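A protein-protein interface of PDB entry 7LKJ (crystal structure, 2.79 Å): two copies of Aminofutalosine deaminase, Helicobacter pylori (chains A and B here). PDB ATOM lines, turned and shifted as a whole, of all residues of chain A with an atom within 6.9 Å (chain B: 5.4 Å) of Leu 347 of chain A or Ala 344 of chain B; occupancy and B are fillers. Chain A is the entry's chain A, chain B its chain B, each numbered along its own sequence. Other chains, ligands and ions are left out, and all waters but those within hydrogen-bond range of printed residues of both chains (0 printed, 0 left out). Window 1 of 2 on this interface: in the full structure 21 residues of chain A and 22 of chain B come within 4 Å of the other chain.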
ATOM      1  N   ASP A 340      12.054 -13.003  23.520  1.00  0.00           N
ATOM      2  CA  ASP A 340      13.450 -13.412  23.403  1.00  0.00           C
ATOM      3  C   ASP A 340      14.350 -12.592  24.307  1.00  0.00           C
ATOM      4  O   ASP A 340      15.392 -13.083  24.753  1.00  0.00           O
ATOM      5  CB  ASP A 340      13.941 -13.282  21.957  1.00  0.00           C
ATOM      6  CG  ASP A 340      13.153 -14.121  20.993  1.00  0.00           C
ATOM      7  OD1 ASP A 340      12.307 -14.908  21.446  1.00  0.00           O
ATOM      8  OD2 ASP A 340      13.382 -13.986  19.762  1.00  0.00           O
ATOM      9  N   LEU A 342      13.385 -11.360  27.186  1.00  0.00           N
ATOM     10  CA  LEU A 342      13.061 -11.804  28.532  1.00  0.00           C
ATOM     11  C   LEU A 342      13.822 -13.072  28.872  1.00  0.00           C
ATOM     12  O   LEU A 342      14.369 -13.193  29.972  1.00  0.00           O
ATOM     13  CB  LEU A 342      11.552 -12.035  28.668  1.00  0.00           C
ATOM     14  CG  LEU A 342      10.677 -10.785  28.823  1.00  0.00           C
ATOM     15  CD1 LEU A 342       9.204 -11.101  28.598  1.00  0.00           C
ATOM     16  CD2 LEU A 342      10.895 -10.195  30.194  1.00  0.00           C
ATOM     17  N   ARG A 343      13.891 -14.014  27.923  1.00  0.00           N
ATOM     18  CA  ARG A 343      14.685 -15.216  28.139  1.00  0.00           C
ATOM     19  C   ARG A 343      16.163 -14.870  28.265  1.00  0.00           C
ATOM     20  O   ARG A 343      16.871 -15.432  29.110  1.00  0.00           O
ATOM     21  CB  ARG A 343      14.456 -16.214  27.006  1.00  0.00           C
ATOM     22  CG  ARG A 343      12.995 -16.476  26.688  1.00  0.00           C
ATOM     23  CD  ARG A 343      12.833 -17.628  25.707  1.00  0.00           C
ATOM     24  NE  ARG A 343      12.432 -17.171  24.378  1.00  0.00           N
ATOM     25  CZ  ARG A 343      11.195 -16.817  24.048  1.00  0.00           C
ATOM     26  NH1 ARG A 343      10.223 -16.865  24.950  1.00  0.00           N
ATOM     27  NH2 ARG A 343      10.925 -16.414  22.814  1.00  0.00           N
ATOM     28  N   ALA A 344      16.649 -13.950  27.427  1.00  0.00           N
ATOM     29  CA  ALA A 344      18.026 -13.487  27.559  1.00  0.00           C
ATOM     30  C   ALA A 344      18.230 -12.726  28.862  1.00  0.00           C
ATOM     31  O   ALA A 344      19.327 -12.755  29.435  1.00  0.00           O
ATOM     32  CB  ALA A 344      18.408 -12.611  26.366  1.00  0.00           C
ATOM     33  N   PHE A 345      17.190 -12.041  29.341  1.00  0.00           N
ATOM     34  CA  PHE A 345      17.245 -11.422  30.660  1.00  0.00           C
ATOM     35  C   PHE A 345      17.363 -12.467  31.762  1.00  0.00           C
ATOM     36  O   PHE A 345      18.030 -12.229  32.775  1.00  0.00           O
ATOM     37  CB  PHE A 345      16.008 -10.550  30.873  1.00  0.00           C
ATOM     38  CG  PHE A 345      15.956  -9.878  32.213  1.00  0.00           C
ATOM     39  CD1 PHE A 345      16.822  -8.841  32.519  1.00  0.00           C
ATOM     40  CD2 PHE A 345      15.030 -10.275  33.162  1.00  0.00           C
ATOM     41  CE1 PHE A 345      16.768  -8.219  33.751  1.00  0.00           C
ATOM     42  CE2 PHE A 345      14.972  -9.657  34.394  1.00  0.00           C
ATOM     43  CZ  PHE A 345      15.840  -8.628  34.689  1.00  0.00           C
ATOM     44  N   LEU A 346      16.730 -13.630  31.579  1.00  0.00           N
ATOM     45  CA  LEU A 346      16.813 -14.686  32.584  1.00  0.00           C
ATOM     46  C   LEU A 346      18.215 -15.280  32.655  1.00  0.00           C
ATOM     47  O   LEU A 346      18.707 -15.589  33.747  1.00  0.00           O
ATOM     48  CB  LEU A 346      15.782 -15.777  32.286  1.00  0.00           C
ATOM     49  CG  LEU A 346      14.313 -15.355  32.174  1.00  0.00           C
ATOM     50  CD1 LEU A 346      13.500 -16.410  31.437  1.00  0.00           C
ATOM     51  CD2 LEU A 346      13.705 -15.068  33.536  1.00  0.00           C
ATOM     52  N   LEU A 347      18.874 -15.449  31.508  1.00  0.00           N
ATOM     53  CA  LEU A 347      20.208 -16.037  31.475  1.00  0.00           C
ATOM     54  C   LEU A 347      21.302 -15.072  31.912  1.00  0.00           C
ATOM     55  O   LEU A 347      22.419 -15.522  32.194  1.00  0.00           O
ATOM     56  CB  LEU A 347      20.536 -16.543  30.066  1.00  0.00           C
ATOM     57  CG  LEU A 347      19.702 -17.675  29.467  1.00  0.00           C
ATOM     58  CD1 LEU A 347      19.556 -17.481  27.966  1.00  0.00           C
ATOM     59  CD2 LEU A 347      20.334 -19.020  29.774  1.00  0.00           C
ATOM     60  N   SER A 348      21.015 -13.774  31.982  1.00  0.00           N
ATOM     61  CA  SER A 348      22.049 -12.769  32.191  1.00  0.00           C
ATOM     62  C   SER A 348      22.296 -12.434  33.657  1.00  0.00           C
ATOM     63  O   SER A 348      23.289 -11.763  33.957  1.00  0.00           O
ATOM     64  CB  SER A 348      21.690 -11.486  31.433  1.00  0.00           C
ATOM     65  OG  SER A 348      21.468 -11.759  30.060  1.00  0.00           O
ATOM     66  N   HIS A 349      21.435 -12.873  34.570  1.00  0.00           N
ATOM     67  CA  HIS A 349      21.580 -12.552  35.983  1.00  0.00           C
ATOM     68  C   HIS A 349      21.552 -13.830  36.809  1.00  0.00           C
ATOM     69  O   HIS A 349      20.822 -14.773  36.488  1.00  0.00           O
ATOM     70  CB  HIS A 349      20.479 -11.595  36.452  1.00  0.00           C
ATOM     71  CG  HIS A 349      20.368 -10.352  35.625  1.00  0.00           C
ATOM     72  ND1 HIS A 349      21.023  -9.182  35.946  1.00  0.00           N
ATOM     73  CD2 HIS A 349      19.676 -10.096  34.490  1.00  0.00           C
ATOM     74  CE1 HIS A 349      20.741  -8.261  35.043  1.00  0.00           C
ATOM     75  NE2 HIS A 349      19.925  -8.788  34.149  1.00  0.00           N
ATOM     76  N   ASN A 350      22.350 -13.851  37.875  1.00  0.00           N
ATOM     77  CA  ASN A 350      22.508 -15.024  38.725  1.00  0.00           C
ATOM     78  C   ASN A 350      21.481 -15.090  39.849  1.00  0.00           C
ATOM     79  O   ASN A 350      21.630 -15.911  40.760  1.00  0.00           O
ATOM     80  CB  ASN A 350      23.920 -15.052  39.315  1.00  0.00           C
ATOM     81  CG  ASN A 350      24.142 -13.962  40.347  1.00  0.00           C
ATOM     82  OD1 ASN A 350      23.891 -14.157  41.536  1.00  0.00           O
ATOM     83  ND2 ASN A 350      24.611 -12.805  39.894  1.00  0.00           N
ATOM     84  N   LEU A 353      16.029 -18.038  40.150  1.00  0.00           N
ATOM     85  CA  LEU A 353      15.276 -17.975  38.898  1.00  0.00           C
ATOM     86  C   LEU A 353      13.815 -17.597  39.119  1.00  0.00           C
ATOM     87  O   LEU A 353      13.264 -16.774  38.377  1.00  0.00           O
ATOM     88  CB  LEU A 353      15.373 -19.317  38.172  1.00  0.00           C
ATOM     89  CG  LEU A 353      14.759 -19.382  36.774  1.00  0.00           C
ATOM     90  CD1 LEU A 353      15.304 -18.265  35.899  1.00  0.00           C
ATOM     91  CD2 LEU A 353      15.015 -20.741  36.141  1.00  0.00           C
ATOM     92  N   LEU A 356      13.433 -13.962  39.954  1.00  0.00           N
ATOM     93  CA  LEU A 356      13.820 -13.128  38.822  1.00  0.00           C
ATOM     94  C   LEU A 356      12.822 -13.229  37.675  1.00  0.00           C
ATOM     95  O   LEU A 356      12.686 -12.283  36.890  1.00  0.00           O
ATOM     96  CB  LEU A 356      15.224 -13.520  38.359  1.00  0.00           C
ATOM     97  CG  LEU A 356      15.823 -12.825  37.139  1.00  0.00           C
ATOM     98  CD1 LEU A 356      17.145 -12.187  37.500  1.00  0.00           C
ATOM     99  CD2 LEU A 356      16.009 -13.822  36.014  1.00  0.00           C
ATOM    100  N   PRO B 300      24.632 -24.861  28.709  1.00  0.00           N
ATOM    101  CA  PRO B 300      24.244 -23.623  29.416  1.00  0.00           C
ATOM    102  C   PRO B 300      22.783 -23.517  29.831  1.00  0.00           C
ATOM    103  O   PRO B 300      22.503 -23.136  30.975  1.00  0.00           O
ATOM    104  CB  PRO B 300      24.624 -22.529  28.403  1.00  0.00           C
ATOM    105  CG  PRO B 300      24.717 -23.235  27.082  1.00  0.00           C
ATOM    106  CD  PRO B 300      25.262 -24.580  27.411  1.00  0.00           C
ATOM    107  N   PHE B 301      21.843 -23.833  28.938  1.00  0.00           N
ATOM    108  CA  PHE B 301      20.435 -23.586  29.244  1.00  0.00           C
ATOM    109  C   PHE B 301      19.917 -24.505  30.347  1.00  0.00           C
ATOM    110  O   PHE B 301      19.143 -24.070  31.207  1.00  0.00           O
ATOM    111  CB  PHE B 301      19.582 -23.728  27.986  1.00  0.00           C
ATOM    112  CG  PHE B 301      18.330 -22.898  28.012  1.00  0.00           C
ATOM    113  CD1 PHE B 301      17.080 -23.494  27.988  1.00  0.00           C
ATOM    114  CD2 PHE B 301      18.406 -21.516  28.074  1.00  0.00           C
ATOM    115  CE1 PHE B 301      15.931 -22.727  28.019  1.00  0.00           C
ATOM    116  CE2 PHE B 301      17.260 -20.744  28.105  1.00  0.00           C
ATOM    117  CZ  PHE B 301      16.021 -21.350  28.077  1.00  0.00           C
ATOM    118  N   ARG B 304      20.706 -23.339  33.885  1.00  0.00           N
ATOM    119  CA  ARG B 304      19.938 -22.199  34.375  1.00  0.00           C
ATOM    120  C   ARG B 304      18.607 -22.646  34.965  1.00  0.00           C
ATOM    121  O   ARG B 304      18.225 -22.218  36.060  1.00  0.00           O
ATOM    122  CB  ARG B 304      19.716 -21.201  33.238  1.00  0.00           C
ATOM    123  CG  ARG B 304      19.257 -19.827  33.685  1.00  0.00           C
ATOM    124  CD  ARG B 304      20.209 -19.233  34.706  1.00  0.00           C
ATOM    125  NE  ARG B 304      19.615 -18.096  35.402  1.00  0.00           N
ATOM    126  CZ  ARG B 304      19.413 -18.049  36.714  1.00  0.00           C
ATOM    127  NH1 ARG B 304      19.758 -19.076  37.477  1.00  0.00           N
ATOM    128  NH2 ARG B 304      18.866 -16.973  37.263  1.00  0.00           N
ATOM    129  N   LEU B 339      22.793 -24.006  17.788  1.00  0.00           N
ATOM    130  CA  LEU B 339      23.107 -22.588  17.645  1.00  0.00           C
ATOM    131  C   LEU B 339      22.446 -21.754  18.739  1.00  0.00           C
ATOM    132  O   LEU B 339      23.081 -20.865  19.316  1.00  0.00           O
ATOM    133  CB  LEU B 339      22.680 -22.096  16.264  1.00  0.00           C
ATOM    134  CG  LEU B 339      23.411 -22.754  15.092  1.00  0.00           C
ATOM    135  CD1 LEU B 339      22.628 -22.584  13.800  1.00  0.00           C
ATOM    136  CD2 LEU B 339      24.817 -22.191  14.953  1.00  0.00           C
ATOM    137  N   ASP B 340      21.175 -22.031  19.041  1.00  0.00           N
ATOM    138  CA  ASP B 340      20.491 -21.317  20.114  1.00  0.00           C
ATOM    139  C   ASP B 340      21.103 -21.618  21.475  1.00  0.00           C
ATOM    140  O   ASP B 340      21.081 -20.760  22.367  1.00  0.00           O
ATOM    141  CB  ASP B 340      19.002 -21.657  20.106  1.00  0.00           C
ATOM    142  CG  ASP B 340      18.344 -21.343  18.776  1.00  0.00           C
ATOM    143  OD1 ASP B 340      17.228 -21.843  18.528  1.00  0.00           O
ATOM    144  OD2 ASP B 340      18.951 -20.598  17.976  1.00  0.00           O
ATOM    145  N   GLU B 341      21.655 -22.820  21.657  1.00  0.00           N
ATOM    146  CA  GLU B 341      22.349 -23.123  22.902  1.00  0.00           C
ATOM    147  C   GLU B 341      23.712 -22.451  22.964  1.00  0.00           C
ATOM    148  O   GLU B 341      24.238 -22.239  24.061  1.00  0.00           O
ATOM    149  CB  GLU B 341      22.503 -24.643  23.046  1.00  0.00           C
ATOM    150  CG  GLU B 341      23.097 -25.106  24.365  1.00  0.00           C
ATOM    151  CD  GLU B 341      22.039 -25.447  25.394  1.00  0.00           C
ATOM    152  OE1 GLU B 341      20.846 -25.502  25.027  1.00  0.00           O
ATOM    153  OE2 GLU B 341      22.398 -25.663  26.570  1.00  0.00           O
ATOM    154  N   LEU B 342      24.280 -22.088  21.813  1.00  0.00           N
ATOM    155  CA  LEU B 342      25.534 -21.347  21.809  1.00  0.00           C
ATOM    156  C   LEU B 342      25.319 -19.900  22.236  1.00  0.00           C
ATOM    157  O   LEU B 342      26.115 -19.350  23.005  1.00  0.00           O
ATOM    158  CB  LEU B 342      26.182 -21.416  20.427  1.00  0.00           C
ATOM    159  CG  LEU B 342      26.800 -22.766  20.051  1.00  0.00           C
ATOM    160  CD1 LEU B 342      27.097 -22.834  18.560  1.00  0.00           C
ATOM    161  CD2 LEU B 342      28.053 -23.048  20.869  1.00  0.00           C
ATOM    162  N   ARG B 343      24.250 -19.264  21.743  1.00  0.00           N
ATOM    163  CA  ARG B 343      23.961 -17.889  22.142  1.00  0.00           C
ATOM    164  C   ARG B 343      23.674 -17.797  23.635  1.00  0.00           C
ATOM    165  O   ARG B 343      24.124 -16.860  24.304  1.00  0.00           O
ATOM    166  CB  ARG B 343      22.783 -17.337  21.340  1.00  0.00           C
ATOM    167  CG  ARG B 343      22.817 -17.659  19.859  1.00  0.00           C
ATOM    168  CD  ARG B 343      21.733 -16.896  19.117  1.00  0.00           C
ATOM    169  NE  ARG B 343      20.840 -17.786  18.382  1.00  0.00           N
ATOM    170  CZ  ARG B 343      21.133 -18.341  17.210  1.00  0.00           C
ATOM    171  NH1 ARG B 343      22.301 -18.098  16.631  1.00  0.00           N
ATOM    172  NH2 ARG B 343      20.257 -19.141  16.616  1.00  0.00           N
ATOM    173  N   ALA B 344      22.925 -18.763  24.175  1.00  0.00           N
ATOM    174  CA  ALA B 344      22.700 -18.795  25.614  1.00  0.00           C
ATOM    175  C   ALA B 344      23.995 -19.063  26.366  1.00  0.00           C
ATOM    176  O   ALA B 344      24.162 -18.599  27.500  1.00  0.00           O
ATOM    177  CB  ALA B 344      21.650 -19.851  25.963  1.00  0.00           C
ATOM    178  N   PHE B 345      24.916 -19.811  25.754  1.00  0.00           N
ATOM    179  CA  PHE B 345      26.247 -19.971  26.325  1.00  0.00           C
ATOM    180  C   PHE B 345      26.991 -18.642  26.356  1.00  0.00           C
ATOM    181  O   PHE B 345      27.756 -18.369  27.288  1.00  0.00           O
ATOM    182  CB  PHE B 345      27.026 -21.015  25.524  1.00  0.00           C
ATOM    183  CG  PHE B 345      28.428 -21.241  26.008  1.00  0.00           C
ATOM    184  CD1 PHE B 345      28.668 -21.929  27.186  1.00  0.00           C
ATOM    185  CD2 PHE B 345      29.507 -20.778  25.275  1.00  0.00           C
ATOM    186  CE1 PHE B 345      29.960 -22.142  27.626  1.00  0.00           C
ATOM    187  CE2 PHE B 345      30.800 -20.988  25.710  1.00  0.00           C
ATOM    188  CZ  PHE B 345      31.027 -21.672  26.886  1.00  0.00           C
ATOM    189  N   LEU B 346      26.772 -17.799  25.342  1.00  0.00           N
ATOM    190  CA  LEU B 346      27.411 -16.486  25.315  1.00  0.00           C
ATOM    191  C   LEU B 346      26.835 -15.569  26.389  1.00  0.00           C
ATOM    192  O   LEU B 346      27.571 -14.795  27.012  1.00  0.00           O
ATOM    193  CB  LEU B 346      27.260 -15.852  23.932  1.00  0.00           C
ATOM    194  CG  LEU B 346      27.756 -16.653  22.722  1.00  0.00           C
ATOM    195  CD1 LEU B 346      27.134 -16.128  21.438  1.00  0.00           C
ATOM    196  CD2 LEU B 346      29.272 -16.627  22.625  1.00  0.00           C
ATOM    197  N   LEU B 347      25.523 -15.641  26.618  1.00  0.00           N
ATOM    198  CA  LEU B 347      24.863 -14.784  27.596  1.00  0.00           C
ATOM    199  C   LEU B 347      25.106 -15.219  29.035  1.00  0.00           C
ATOM    200  O   LEU B 347      24.826 -14.441  29.952  1.00  0.00           O
ATOM    201  CB  LEU B 347      23.353 -14.750  27.333  1.00  0.00           C
ATOM    202  CG  LEU B 347      22.871 -14.282  25.959  1.00  0.00           C
ATOM    203  CD1 LEU B 347      21.629 -15.056  25.538  1.00  0.00           C
ATOM    204  CD2 LEU B 347      22.594 -12.787  25.969  1.00  0.00           C
ATOM    205  N   SER B 348      25.611 -16.432  29.255  1.00  0.00           N
ATOM    206  CA  SER B 348      25.704 -17.001  30.592  1.00  0.00           C
ATOM    207  C   SER B 348      27.031 -16.727  31.291  1.00  0.00           C
ATOM    208  O   SER B 348      27.138 -16.983  32.495  1.00  0.00           O
ATOM    209  CB  SER B 348      25.471 -18.514  30.533  1.00  0.00           C
ATOM    210  OG  SER B 348      24.270 -18.815  29.845  1.00  0.00           O
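Leu 347 of chain A touches Ala 344 of chain B, but with the chains exchanged Ala 344 of chain A does not touch Leu 347 of chain B (4.1 Å).
Leu 347 of chain A touches its own counterpart, Leu 347 of chain B.
Leu 347 of chain A touches Ser 348 of chain B, and with the chains exchanged Ser 348 of chain A touches Leu 347 of chain B.
Of the 8 pairs that touch across the chains among the printed residues, 3 have their exchanged pair printed and touching as well.
The backbone carbonyl oxygen of Ala 344 of chain A sits at hydrogen-bond distance from the side-chain hydroxyl of Ser 348 of chain A.
The side-chain carboxylate of Glu 341 of chain B lies within hydrogen-bond range of the backbone NH of Phe 301 of chain B (3.0 Å).
CD2 of Phe 301 of chain B touches CD2 of Leu 347 of chain A (3.6 Å).
Leu 347 of chain A touches Ala 344 of chain B (CD1 to CB, 3.7 Å).
Leu 347 of chain A touches Ser 348 of chain B.
Ser 348 of chain A touches Leu 347 of chain B (CA to O, 3.9 Å).
Leu 353 of chain A touches Arg 304 of chain B (CD2 to O, 3.5 Å).
Hydrophobic or aromatic side chains of chain A that line the printed part of chain B: Leu 347 and Leu 353.
Printed residues of chain B that touch a printed residue of chain A: Phe 301, Arg 304, Ala 344, Leu 347 and Ser 348.
Among the printed residues, no Asp or Glu carboxylate lies within 4 Å of a Lys or Arg side-chain nitrogen of the other chain.
The backbone carbonyl oxygen (O) of Leu 346 of chain A is in hydrogen-bond range of the guanidinium group (NE) of Arg 304 of chain B (3.1 Å).
The guanidinium group (NH2) of Arg 304 of chain B lies within hydrogen-bond range of the backbone carbonyl oxygen (O) of His 349 of chain A (3.0 Å).
O of Leu 347 of chain B lies close to O of Leu 347 of chain A, 3.5 Å away.
Of the printed residues of chain B, Leu 347 of chain A touches Phe 301 (3.6 Å), Ala 344 (3.7 Å), Leu 347 (3.5 Å) and Ser 348 (3.9 Å).
Printed residues of chain A within 4 Å of Phe 301 of chain B: Leu 347.
Printed residues of chain B within 4 Å of His 349 of chain A: Arg 304 (3.0 Å).
Printed residues of chain B within 4 Å of Leu 346 of chain A: Arg 304.
Printed residues of chain A within 4 Å of Leu 347 of chain B: Leu 347 and Ser 348.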
